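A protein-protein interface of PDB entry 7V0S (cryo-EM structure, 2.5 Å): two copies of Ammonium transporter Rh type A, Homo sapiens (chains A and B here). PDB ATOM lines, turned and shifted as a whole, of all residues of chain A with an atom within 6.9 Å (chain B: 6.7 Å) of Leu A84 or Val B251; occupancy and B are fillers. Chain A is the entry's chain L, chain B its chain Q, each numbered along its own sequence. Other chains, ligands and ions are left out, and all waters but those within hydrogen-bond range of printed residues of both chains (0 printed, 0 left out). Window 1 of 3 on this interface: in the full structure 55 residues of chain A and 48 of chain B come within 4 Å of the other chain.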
ATOM      1  N   GLU A  13       1.517  28.391  -6.155  1.00  0.00           N
ATOM      2  CA  GLU A  13       1.220  27.015  -5.768  1.00  0.00           C
ATOM      3  C   GLU A  13       1.025  26.886  -4.260  1.00  0.00           C
ATOM      4  O   GLU A  13       0.146  26.145  -3.805  1.00  0.00           O
ATOM      5  CB  GLU A  13       2.324  26.078  -6.249  1.00  0.00           C
ATOM      6  CG  GLU A  13       1.983  24.616  -6.050  1.00  0.00           C
ATOM      7  CD  GLU A  13       0.675  24.238  -6.718  1.00  0.00           C
ATOM      8  OE1 GLU A  13       0.542  24.470  -7.936  1.00  0.00           O
ATOM      9  OE2 GLU A  13      -0.225  23.723  -6.027  1.00  0.00           O
ATOM     10  N   ILE A  61      -8.934  20.229 -23.248  1.00  0.00           N
ATOM     11  CA  ILE A  61      -8.192  21.323 -22.628  1.00  0.00           C
ATOM     12  C   ILE A  61      -6.705  21.201 -22.926  1.00  0.00           C
ATOM     13  O   ILE A  61      -6.062  22.165 -23.355  1.00  0.00           O
ATOM     14  CB  ILE A  61      -8.450  21.368 -21.109  1.00  0.00           C
ATOM     15  CG1 ILE A  61      -9.926  21.624 -20.815  1.00  0.00           C
ATOM     16  CG2 ILE A  61      -7.585  22.429 -20.451  1.00  0.00           C
ATOM     17  CD1 ILE A  61     -10.540  22.677 -21.670  1.00  0.00           C
ATOM     18  N   PHE A  62      -6.137  20.015 -22.721  1.00  0.00           N
ATOM     19  CA  PHE A  62      -4.682  19.937 -22.718  1.00  0.00           C
ATOM     20  C   PHE A  62      -4.096  19.514 -24.060  1.00  0.00           C
ATOM     21  O   PHE A  62      -3.053  20.038 -24.463  1.00  0.00           O
ATOM     22  CB  PHE A  62      -4.220  19.002 -21.599  1.00  0.00           C
ATOM     23  CG  PHE A  62      -4.417  19.584 -20.233  1.00  0.00           C
ATOM     24  CD1 PHE A  62      -3.430  20.363 -19.654  1.00  0.00           C
ATOM     25  CD2 PHE A  62      -5.607  19.400 -19.551  1.00  0.00           C
ATOM     26  CE1 PHE A  62      -3.614  20.917 -18.407  1.00  0.00           C
ATOM     27  CE2 PHE A  62      -5.798  19.958 -18.307  1.00  0.00           C
ATOM     28  CZ  PHE A  62      -4.801  20.722 -17.735  1.00  0.00           C
ATOM     29  N   GLY A  66      -3.688  23.137 -26.781  1.00  0.00           N
ATOM     30  CA  GLY A  66      -2.239  23.237 -26.756  1.00  0.00           C
ATOM     31  C   GLY A  66      -1.604  22.887 -28.084  1.00  0.00           C
ATOM     32  O   GLY A  66      -0.736  23.607 -28.580  1.00  0.00           O
ATOM     33  N   SER A  78       6.627  26.723 -26.467  1.00  0.00           N
ATOM     34  CA  SER A  78       5.885  27.658 -25.635  1.00  0.00           C
ATOM     35  C   SER A  78       4.389  27.410 -25.732  1.00  0.00           C
ATOM     36  O   SER A  78       3.700  27.405 -24.713  1.00  0.00           O
ATOM     37  CB  SER A  78       6.217  29.094 -26.028  1.00  0.00           C
ATOM     38  OG  SER A  78       7.534  29.439 -25.648  1.00  0.00           O
ATOM     39  N   SER A  79       3.883  27.146 -26.937  1.00  0.00           N
ATOM     40  CA  SER A  79       2.458  26.875 -27.107  1.00  0.00           C
ATOM     41  C   SER A  79       2.004  25.733 -26.206  1.00  0.00           C
ATOM     42  O   SER A  79       1.207  25.936 -25.282  1.00  0.00           O
ATOM     43  CB  SER A  79       2.153  26.563 -28.572  1.00  0.00           C
ATOM     44  OG  SER A  79       2.015  27.752 -29.321  1.00  0.00           O
ATOM     45  N   VAL A  80       2.556  24.537 -26.413  1.00  0.00           N
ATOM     46  CA  VAL A  80       2.055  23.377 -25.683  1.00  0.00           C
ATOM     47  C   VAL A  80       2.423  23.455 -24.197  1.00  0.00           C
ATOM     48  O   VAL A  80       1.593  23.152 -23.327  1.00  0.00           O
ATOM     49  CB  VAL A  80       2.529  22.072 -26.360  1.00  0.00           C
ATOM     50  CG1 VAL A  80       4.025  21.846 -26.207  1.00  0.00           C
ATOM     51  CG2 VAL A  80       1.746  20.888 -25.828  1.00  0.00           C
ATOM     52  N   GLY A  81       3.638  23.909 -23.870  1.00  0.00           N
ATOM     53  CA  GLY A  81       4.057  23.932 -22.480  1.00  0.00           C
ATOM     54  C   GLY A  81       3.347  24.984 -21.650  1.00  0.00           C
ATOM     55  O   GLY A  81       2.916  24.708 -20.530  1.00  0.00           O
ATOM     56  N   ILE A  82       3.234  26.209 -22.171  1.00  0.00           N
ATOM     57  CA  ILE A  82       2.512  27.245 -21.454  1.00  0.00           C
ATOM     58  C   ILE A  82       1.024  26.929 -21.427  1.00  0.00           C
ATOM     59  O   ILE A  82       0.334  27.291 -20.473  1.00  0.00           O
ATOM     60  CB  ILE A  82       2.818  28.630 -22.062  1.00  0.00           C
ATOM     61  CG1 ILE A  82       4.326  28.905 -22.035  1.00  0.00           C
ATOM     62  CG2 ILE A  82       2.095  29.735 -21.319  1.00  0.00           C
ATOM     63  CD1 ILE A  82       4.981  28.666 -20.689  1.00  0.00           C
ATOM     64  N   ASN A  83       0.505  26.212 -22.432  1.00  0.00           N
ATOM     65  CA  ASN A  83      -0.852  25.685 -22.326  1.00  0.00           C
ATOM     66  C   ASN A  83      -0.989  24.781 -21.108  1.00  0.00           C
ATOM     67  O   ASN A  83      -1.905  24.949 -20.295  1.00  0.00           O
ATOM     68  CB  ASN A  83      -1.213  24.921 -23.601  1.00  0.00           C
ATOM     69  CG  ASN A  83      -2.688  24.577 -23.684  1.00  0.00           C
ATOM     70  OD1 ASN A  83      -3.477  25.328 -24.250  1.00  0.00           O
ATOM     71  ND2 ASN A  83      -3.064  23.432 -23.131  1.00  0.00           N
ATOM     72  N   LEU A  84      -0.063  23.831 -20.957  1.00  0.00           N
ATOM     73  CA  LEU A  84      -0.112  22.911 -19.822  1.00  0.00           C
ATOM     74  C   LEU A  84       0.011  23.657 -18.496  1.00  0.00           C
ATOM     75  O   LEU A  84      -0.752  23.406 -17.557  1.00  0.00           O
ATOM     76  CB  LEU A  84       0.991  21.863 -19.957  1.00  0.00           C
ATOM     77  CG  LEU A  84       1.284  20.999 -18.729  1.00  0.00           C
ATOM     78  CD1 LEU A  84       0.105  20.093 -18.401  1.00  0.00           C
ATOM     79  CD2 LEU A  84       2.551  20.189 -18.936  1.00  0.00           C
ATOM     80  N   LEU A  85       0.953  24.596 -18.414  1.00  0.00           N
ATOM     81  CA  LEU A  85       1.182  25.336 -17.175  1.00  0.00           C
ATOM     82  C   LEU A  85      -0.015  26.211 -16.818  1.00  0.00           C
ATOM     83  O   LEU A  85      -0.483  26.210 -15.668  1.00  0.00           O
ATOM     84  CB  LEU A  85       2.449  26.181 -17.313  1.00  0.00           C
ATOM     85  CG  LEU A  85       2.699  27.291 -16.293  1.00  0.00           C
ATOM     86  CD1 LEU A  85       3.053  26.709 -14.938  1.00  0.00           C
ATOM     87  CD2 LEU A  85       3.793  28.220 -16.781  1.00  0.00           C
ATOM     88  N   VAL A  86      -0.526  26.959 -17.797  1.00  0.00           N
ATOM     89  CA  VAL A  86      -1.655  27.850 -17.576  1.00  0.00           C
ATOM     90  C   VAL A  86      -2.880  27.058 -17.154  1.00  0.00           C
ATOM     91  O   VAL A  86      -3.572  27.434 -16.205  1.00  0.00           O
ATOM     92  CB  VAL A  86      -1.924  28.689 -18.841  1.00  0.00           C
ATOM     93  CG1 VAL A  86      -3.382  29.093 -18.926  1.00  0.00           C
ATOM     94  CG2 VAL A  86      -1.038  29.913 -18.854  1.00  0.00           C
ATOM     95  N   ALA A  87      -3.153  25.935 -17.822  1.00  0.00           N
ATOM     96  CA  ALA A  87      -4.347  25.170 -17.485  1.00  0.00           C
ATOM     97  C   ALA A  87      -4.193  24.444 -16.151  1.00  0.00           C
ATOM     98  O   ALA A  87      -5.177  24.270 -15.424  1.00  0.00           O
ATOM     99  CB  ALA A  87      -4.675  24.194 -18.611  1.00  0.00           C
ATOM    100  N   ALA A  88      -2.973  24.020 -15.804  1.00  0.00           N
ATOM    101  CA  ALA A  88      -2.760  23.378 -14.511  1.00  0.00           C
ATOM    102  C   ALA A  88      -2.960  24.358 -13.362  1.00  0.00           C
ATOM    103  O   ALA A  88      -3.578  24.016 -12.349  1.00  0.00           O
ATOM    104  CB  ALA A  88      -1.365  22.759 -14.450  1.00  0.00           C
ATOM    105  N   LEU A  89      -2.434  25.578 -13.493  1.00  0.00           N
ATOM    106  CA  LEU A  89      -2.739  26.606 -12.502  1.00  0.00           C
ATOM    107  C   LEU A  89      -4.223  26.949 -12.524  1.00  0.00           C
ATOM    108  O   LEU A  89      -4.842  27.187 -11.472  1.00  0.00           O
ATOM    109  CB  LEU A  89      -1.898  27.856 -12.763  1.00  0.00           C
ATOM    110  CG  LEU A  89      -2.230  29.092 -11.924  1.00  0.00           C
ATOM    111  CD1 LEU A  89      -2.072  28.800 -10.437  1.00  0.00           C
ATOM    112  CD2 LEU A  89      -1.373  30.272 -12.335  1.00  0.00           C
ATOM    113  N   GLY A  90      -4.808  26.961 -13.721  1.00  0.00           N
ATOM    114  CA  GLY A  90      -6.169  27.417 -13.879  1.00  0.00           C
ATOM    115  C   GLY A  90      -7.189  26.498 -13.249  1.00  0.00           C
ATOM    116  O   GLY A  90      -8.176  26.964 -12.691  1.00  0.00           O
ATOM    117  N   LEU A  91      -6.981  25.187 -13.346  1.00  0.00           N
ATOM    118  CA  LEU A  91      -7.950  24.271 -12.755  1.00  0.00           C
ATOM    119  C   LEU A  91      -7.989  24.418 -11.237  1.00  0.00           C
ATOM    120  O   LEU A  91      -9.070  24.448 -10.643  1.00  0.00           O
ATOM    121  CB  LEU A  91      -7.657  22.831 -13.187  1.00  0.00           C
ATOM    122  CG  LEU A  91      -6.432  22.044 -12.730  1.00  0.00           C
ATOM    123  CD1 LEU A  91      -6.702  21.312 -11.429  1.00  0.00           C
ATOM    124  CD2 LEU A  91      -6.030  21.067 -13.827  1.00  0.00           C
ATOM    125  N   GLN A  92      -6.827  24.578 -10.599  1.00  0.00           N
ATOM    126  CA  GLN A  92      -6.791  24.786  -9.152  1.00  0.00           C
ATOM    127  C   GLN A  92      -7.454  26.103  -8.762  1.00  0.00           C
ATOM    128  O   GLN A  92      -8.337  26.142  -7.889  1.00  0.00           O
ATOM    129  CB  GLN A  92      -5.343  24.751  -8.662  1.00  0.00           C
ATOM    130  CG  GLN A  92      -4.612  23.466  -8.978  1.00  0.00           C
ATOM    131  CD  GLN A  92      -3.113  23.572  -8.759  1.00  0.00           C
ATOM    132  OE1 GLN A  92      -2.615  23.327  -7.664  1.00  0.00           O
ATOM    133  NE2 GLN A  92      -2.389  23.939  -9.806  1.00  0.00           N
ATOM    134  N   LEU A 126      -7.268  29.698 -21.732  1.00  0.00           N
ATOM    135  CA  LEU A 126      -6.521  29.291 -22.921  1.00  0.00           C
ATOM    136  C   LEU A 126      -7.016  30.020 -24.168  1.00  0.00           C
ATOM    137  O   LEU A 126      -6.220  30.366 -25.052  1.00  0.00           O
ATOM    138  CB  LEU A 126      -6.612  27.779 -23.103  1.00  0.00           C
ATOM    139  CG  LEU A 126      -5.896  26.966 -22.025  1.00  0.00           C
ATOM    140  CD1 LEU A 126      -6.088  25.477 -22.242  1.00  0.00           C
ATOM    141  CD2 LEU A 126      -4.420  27.331 -21.965  1.00  0.00           C
ATOM    142  N   PHE A 129      -5.406  33.225 -24.017  1.00  0.00           N
ATOM    143  CA  PHE A 129      -3.996  33.024 -24.337  1.00  0.00           C
ATOM    144  C   PHE A 129      -3.772  33.003 -25.842  1.00  0.00           C
ATOM    145  O   PHE A 129      -2.758  33.507 -26.335  1.00  0.00           O
ATOM    146  CB  PHE A 129      -3.516  31.719 -23.695  1.00  0.00           C
ATOM    147  CG  PHE A 129      -2.076  31.365 -23.977  1.00  0.00           C
ATOM    148  CD1 PHE A 129      -1.090  32.337 -24.055  1.00  0.00           C
ATOM    149  CD2 PHE A 129      -1.708  30.042 -24.132  1.00  0.00           C
ATOM    150  CE1 PHE A 129       0.223  31.997 -24.296  1.00  0.00           C
ATOM    151  CE2 PHE A 129      -0.396  29.696 -24.372  1.00  0.00           C
ATOM    152  CZ  PHE A 129       0.569  30.675 -24.450  1.00  0.00           C
ATOM    153  N   MET B 212       5.876  15.588 -26.220  1.00  0.00           N
ATOM    154  CA  MET B 212       4.825  16.309 -25.512  1.00  0.00           C
ATOM    155  C   MET B 212       3.462  15.658 -25.708  1.00  0.00           C
ATOM    156  O   MET B 212       2.632  15.696 -24.796  1.00  0.00           O
ATOM    157  CB  MET B 212       4.791  17.770 -25.954  1.00  0.00           C
ATOM    158  CG  MET B 212       5.763  18.645 -25.192  1.00  0.00           C
ATOM    159  SD  MET B 212       5.699  18.348 -23.415  1.00  0.00           S
ATOM    160  CE  MET B 212       4.128  19.090 -22.995  1.00  0.00           C
ATOM    161  N   THR B 215       3.593  12.918 -23.158  1.00  0.00           N
ATOM    162  CA  THR B 215       3.517  13.507 -21.825  1.00  0.00           C
ATOM    163  C   THR B 215       2.093  13.913 -21.486  1.00  0.00           C
ATOM    164  O   THR B 215       1.598  13.624 -20.390  1.00  0.00           O
ATOM    165  CB  THR B 215       4.441  14.725 -21.738  1.00  0.00           C
ATOM    166  OG1 THR B 215       5.804  14.301 -21.771  1.00  0.00           O
ATOM    167  CG2 THR B 215       4.185  15.514 -20.460  1.00  0.00           C
ATOM    168  N   LEU B 216       1.420  14.587 -22.417  1.00  0.00           N
ATOM    169  CA  LEU B 216       0.078  15.077 -22.141  1.00  0.00           C
ATOM    170  C   LEU B 216      -0.908  13.934 -21.979  1.00  0.00           C
ATOM    171  O   LEU B 216      -1.790  13.999 -21.119  1.00  0.00           O
ATOM    172  CB  LEU B 216      -0.374  16.033 -23.240  1.00  0.00           C
ATOM    173  CG  LEU B 216       0.289  17.405 -23.172  1.00  0.00           C
ATOM    174  CD1 LEU B 216      -0.306  18.317 -24.218  1.00  0.00           C
ATOM    175  CD2 LEU B 216       0.159  18.008 -21.782  1.00  0.00           C
ATOM    176  N   TRP B 219      -0.306  12.479 -18.540  1.00  0.00           N
ATOM    177  CA  TRP B 219      -0.741  13.426 -17.521  1.00  0.00           C
ATOM    178  C   TRP B 219      -2.257  13.471 -17.408  1.00  0.00           C
ATOM    179  O   TRP B 219      -2.805  13.544 -16.302  1.00  0.00           O
ATOM    180  CB  TRP B 219      -0.192  14.810 -17.858  1.00  0.00           C
ATOM    181  CG  TRP B 219      -0.278  15.796 -16.759  1.00  0.00           C
ATOM    182  CD1 TRP B 219       0.657  16.036 -15.804  1.00  0.00           C
ATOM    183  CD2 TRP B 219      -1.354  16.703 -16.508  1.00  0.00           C
ATOM    184  NE1 TRP B 219       0.227  17.027 -14.961  1.00  0.00           N
ATOM    185  CE2 TRP B 219      -1.005  17.458 -15.374  1.00  0.00           C
ATOM    186  CE3 TRP B 219      -2.580  16.947 -17.130  1.00  0.00           C
ATOM    187  CZ2 TRP B 219      -1.836  18.441 -14.848  1.00  0.00           C
ATOM    188  CZ3 TRP B 219      -3.403  17.917 -16.607  1.00  0.00           C
ATOM    189  CH2 TRP B 219      -3.028  18.656 -15.479  1.00  0.00           C
ATOM    190  N   SER B 246      -2.774  16.514  -7.464  1.00  0.00           N
ATOM    191  CA  SER B 246      -1.340  16.291  -7.326  1.00  0.00           C
ATOM    192  C   SER B 246      -0.614  16.605  -8.627  1.00  0.00           C
ATOM    193  O   SER B 246       0.438  17.253  -8.621  1.00  0.00           O
ATOM    194  CB  SER B 246      -1.081  14.849  -6.891  1.00  0.00           C
ATOM    195  OG  SER B 246       0.302  14.588  -6.778  1.00  0.00           O
ATOM    196  N   LEU B 247      -1.175  16.169  -9.760  1.00  0.00           N
ATOM    197  CA  LEU B 247      -0.573  16.489 -11.050  1.00  0.00           C
ATOM    198  C   LEU B 247      -0.623  17.987 -11.328  1.00  0.00           C
ATOM    199  O   LEU B 247       0.333  18.557 -11.878  1.00  0.00           O
ATOM    200  CB  LEU B 247      -1.273  15.710 -12.159  1.00  0.00           C
ATOM    201  CG  LEU B 247      -0.894  14.234 -12.256  1.00  0.00           C
ATOM    202  CD1 LEU B 247      -1.954  13.479 -13.021  1.00  0.00           C
ATOM    203  CD2 LEU B 247       0.466  14.063 -12.911  1.00  0.00           C
ATOM    204  N   ALA B 248      -1.727  18.641 -10.951  1.00  0.00           N
ATOM    205  CA  ALA B 248      -1.827  20.085 -11.147  1.00  0.00           C
ATOM    206  C   ALA B 248      -0.738  20.834 -10.382  1.00  0.00           C
ATOM    207  O   ALA B 248      -0.109  21.755 -10.918  1.00  0.00           O
ATOM    208  CB  ALA B 248      -3.211  20.576 -10.732  1.00  0.00           C
ATOM    209  N   ALA B 249      -0.503  20.459  -9.122  1.00  0.00           N
ATOM    210  CA  ALA B 249       0.566  21.096  -8.348  1.00  0.00           C
ATOM    211  C   ALA B 249       1.946  20.740  -8.899  1.00  0.00           C
ATOM    212  O   ALA B 249       2.872  21.576  -8.899  1.00  0.00           O
ATOM    213  CB  ALA B 249       0.454  20.690  -6.880  1.00  0.00           C
ATOM    214  N   CYS B 250       2.097  19.499  -9.366  1.00  0.00           N
ATOM    215  CA  CYS B 250       3.375  19.025  -9.874  1.00  0.00           C
ATOM    216  C   CYS B 250       3.807  19.807 -11.103  1.00  0.00           C
ATOM    217  O   CYS B 250       4.998  20.075 -11.283  1.00  0.00           O
ATOM    218  CB  CYS B 250       3.277  17.536 -10.191  1.00  0.00           C
ATOM    219  SG  CYS B 250       4.810  16.773 -10.706  1.00  0.00           S
ATOM    220  N   VAL B 251       2.855  20.176 -11.966  1.00  0.00           N
ATOM    221  CA  VAL B 251       3.203  20.961 -13.152  1.00  0.00           C
ATOM    222  C   VAL B 251       3.818  22.295 -12.746  1.00  0.00           C
ATOM    223  O   VAL B 251       4.848  22.718 -13.291  1.00  0.00           O
ATOM    224  CB  VAL B 251       1.970  21.162 -14.050  1.00  0.00           C
ATOM    225  CG1 VAL B 251       2.191  22.328 -15.005  1.00  0.00           C
ATOM    226  CG2 VAL B 251       1.682  19.909 -14.826  1.00  0.00           C
ATOM    227  N   LEU B 252       3.201  22.971 -11.775  1.00  0.00           N
ATOM    228  CA  LEU B 252       3.693  24.275 -11.343  1.00  0.00           C
ATOM    229  C   LEU B 252       5.097  24.167 -10.770  1.00  0.00           C
ATOM    230  O   LEU B 252       5.989  24.951 -11.120  1.00  0.00           O
ATOM    231  CB  LEU B 252       2.744  24.886 -10.311  1.00  0.00           C
ATOM    232  CG  LEU B 252       1.586  25.774 -10.777  1.00  0.00           C
ATOM    233  CD1 LEU B 252       2.097  27.113 -11.274  1.00  0.00           C
ATOM    234  CD2 LEU B 252       0.724  25.089 -11.832  1.00  0.00           C
ATOM    235  N   THR B 253       5.323  23.180  -9.900  1.00  0.00           N
ATOM    236  CA  THR B 253       6.647  23.089  -9.288  1.00  0.00           C
ATOM    237  C   THR B 253       7.697  22.612 -10.286  1.00  0.00           C
ATOM    238  O   THR B 253       8.858  23.035 -10.216  1.00  0.00           O
ATOM    239  CB  THR B 253       6.612  22.194  -8.055  1.00  0.00           C
ATOM    240  OG1 THR B 253       5.957  20.959  -8.363  1.00  0.00           O
ATOM    241  CG2 THR B 253       5.888  22.910  -6.937  1.00  0.00           C
ATOM    242  N   ALA B 254       7.314  21.750 -11.231  1.00  0.00           N
ATOM    243  CA  ALA B 254       8.248  21.327 -12.266  1.00  0.00           C
ATOM    244  C   ALA B 254       8.673  22.499 -13.139  1.00  0.00           C
ATOM    245  O   ALA B 254       9.863  22.656 -13.428  1.00  0.00           O
ATOM    246  CB  ALA B 254       7.627  20.218 -13.117  1.00  0.00           C
ATOM    247  N   PHE B 255       7.722  23.344 -13.548  1.00  0.00           N
ATOM    248  CA  PHE B 255       8.070  24.524 -14.334  1.00  0.00           C
ATOM    249  C   PHE B 255       8.963  25.470 -13.540  1.00  0.00           C
ATOM    250  O   PHE B 255       9.967  25.981 -14.058  1.00  0.00           O
ATOM    251  CB  PHE B 255       6.804  25.246 -14.793  1.00  0.00           C
ATOM    252  CG  PHE B 255       6.359  24.876 -16.175  1.00  0.00           C
ATOM    253  CD1 PHE B 255       5.510  23.800 -16.381  1.00  0.00           C
ATOM    254  CD2 PHE B 255       6.789  25.602 -17.272  1.00  0.00           C
ATOM    255  CE1 PHE B 255       5.099  23.458 -17.652  1.00  0.00           C
ATOM    256  CE2 PHE B 255       6.378  25.263 -18.547  1.00  0.00           C
ATOM    257  CZ  PHE B 255       5.532  24.191 -18.736  1.00  0.00           C
ATOM    258  N   ALA B 256       8.619  25.701 -12.268  1.00  0.00           N
ATOM    259  CA  ALA B 256       9.390  26.627 -11.444  1.00  0.00           C
ATOM    260  C   ALA B 256      10.827  26.150 -11.267  1.00  0.00           C
ATOM    261  O   ALA B 256      11.777  26.921 -11.441  1.00  0.00           O
ATOM    262  CB  ALA B 256       8.711  26.806 -10.087  1.00  0.00           C
ATOM    263  N   ILE B 272       9.933  19.453 -18.579  1.00  0.00           N
ATOM    264  CA  ILE B 272       8.508  19.626 -18.848  1.00  0.00           C
ATOM    265  C   ILE B 272       7.879  18.320 -19.317  1.00  0.00           C
ATOM    266  O   ILE B 272       6.723  18.026 -18.993  1.00  0.00           O
ATOM    267  CB  ILE B 272       8.305  20.767 -19.861  1.00  0.00           C
ATOM    268  CG1 ILE B 272       8.952  22.047 -19.331  1.00  0.00           C
ATOM    269  CG2 ILE B 272       6.828  20.990 -20.146  1.00  0.00           C
ATOM    270  CD1 ILE B 272       8.568  22.392 -17.910  1.00  0.00           C
ATOM    271  N   ALA B 275       9.127  15.582 -15.558  1.00  0.00           N
ATOM    272  CA  ALA B 275       8.912  15.964 -14.171  1.00  0.00           C
ATOM    273  C   ALA B 275       7.481  16.394 -13.888  1.00  0.00           C
ATOM    274  O   ALA B 275       7.097  16.469 -12.721  1.00  0.00           O
ATOM    275  CB  ALA B 275       9.871  17.089 -13.792  1.00  0.00           C
ATOM    276  N   THR B 276       6.689  16.683 -14.922  1.00  0.00           N
ATOM    277  CA  THR B 276       5.292  17.041 -14.722  1.00  0.00           C
ATOM    278  C   THR B 276       4.410  15.836 -14.414  1.00  0.00           C
ATOM    279  O   THR B 276       3.247  16.025 -14.048  1.00  0.00           O
ATOM    280  CB  THR B 276       4.762  17.777 -15.954  1.00  0.00           C
ATOM    281  OG1 THR B 276       5.028  17.004 -17.129  1.00  0.00           O
ATOM    282  CG2 THR B 276       5.431  19.135 -16.089  1.00  0.00           C
ATOM    283  N   LEU B 277       4.927  14.616 -14.557  1.00  0.00           N
ATOM    284  CA  LEU B 277       4.215  13.400 -14.183  1.00  0.00           C
ATOM    285  C   LEU B 277       4.640  12.867 -12.821  1.00  0.00           C
ATOM    286  O   LEU B 277       4.110  11.838 -12.369  1.00  0.00           O
ATOM    287  CB  LEU B 277       4.438  12.319 -15.248  1.00  0.00           C
ATOM    288  CG  LEU B 277       4.394  12.828 -16.689  1.00  0.00           C
ATOM    289  CD1 LEU B 277       4.947  11.792 -17.650  1.00  0.00           C
ATOM    290  CD2 LEU B 277       2.981  13.214 -17.066  1.00  0.00           C
ATOM    291  N   GLY B 279       4.078  14.091  -9.885  1.00  0.00           N
ATOM    292  CA  GLY B 279       2.983  14.135  -8.930  1.00  0.00           C
ATOM    293  C   GLY B 279       2.052  12.946  -9.058  1.00  0.00           C
ATOM    294  O   GLY B 279       1.571  12.411  -8.059  1.00  0.00           O
ATOM    295  N   GLY B 300       2.473  16.383  -4.726  1.00  0.00           N
ATOM    296  CA  GLY B 300       2.727  16.744  -6.128  1.00  0.00           C
ATOM    297  C   GLY B 300       3.772  17.827  -6.272  1.00  0.00           C
ATOM    298  O   GLY B 300       4.629  17.691  -7.136  1.00  0.00           O
ATOM    299  N   GLY B 304       7.353  17.118  -8.075  1.00  0.00           N
ATOM    300  CA  GLY B 304       7.888  17.890  -9.188  1.00  0.00           C
ATOM    301  C   GLY B 304       9.249  18.484  -8.883  1.00  0.00           C
ATOM    302  O   GLY B 304      10.162  18.437  -9.717  1.00  0.00           O
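O of Ala B248 lies within hydrogen-bond range of NE2 of Gln A92.
OE2 of Glu A13 touches CB of Ala B249, 3.2 Å away. Val A80 touches Met B212. Val A80 touches Leu B216 (CG2 to CD1, 3.7 Å). Leu B216 touches Leu A84. Val B251 touches Leu A84 (CG2 to CD1, 3.9 Å). Leu A85 touches Leu B252 (CD1 to CD1, 3.8 Å). CE1 of Phe B255 touches CB of Leu A85, at 3.8 Å. CB of Ala B248 touches O of Ala A88, 3.8 Å away. Ala A88 touches Val B251 (CB to CG1, 3.6 Å). CD2 of Leu B252 touches N of Leu A89 (3.6 Å).
OE1 of Gln A92 sits close to OE2 of Glu A13 (2.9 Å). The backbone carbonyl oxygen (O) of Ala A88 lies within hydrogen-bond range of the side-chain amide nitrogen (NE2) of Gln A92, at 2.8 Å. The backbone carbonyl oxygen (O) of Leu B247 sits close to the indole nitrogen (NE1) of Trp B219 (3.4 Å). The backbone carbonyl oxygen (O) of Thr B276 lies close to the indole nitrogen (NE1) of Trp B219 (3.3 Å). O of Ala B249 lies within hydrogen-bond range of OG1 of Thr B253 (3.2 Å).
Of the 21 printed residues of chain A, 10 touch a printed residue of chain B. Of the 22 printed residues of chain B, 8 touch a printed residue of chain A. Hydrophobic or aromatic side chains of chain B that line the printed part of chain A: Met B212, Leu B216, Trp B219, Ala B248, Ala B249, Val B251, Leu B252 and Phe B255. Among the printed residues, 19 pairs touch across the chains.
No position is printed for both chains.
Printed residues of chain B within 4 Å of Val A80: Met B212 (3.8 Å) and Leu B216 (3.7 Å). Leu A84 touches just these residues of chain B: Leu B216 and Val B251. Of the printed residues of chain B, Leu A89 touches Leu B252. Of the printed residues of chain A, Ala B249 touches Glu A13 (3.2 Å) and Gln A92 (3.8 Å). Of the printed residues of chain A, Phe B255 touches Gly A81 (3.2 Å) and Leu A85 (3.8 Å). The nearest residue of chain A that does not touch Val B251 is Leu A89 (5.9 Å). The nearest printed residue of chain A that does not touch Ala B248 is Glu A13 (4.1 Å).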
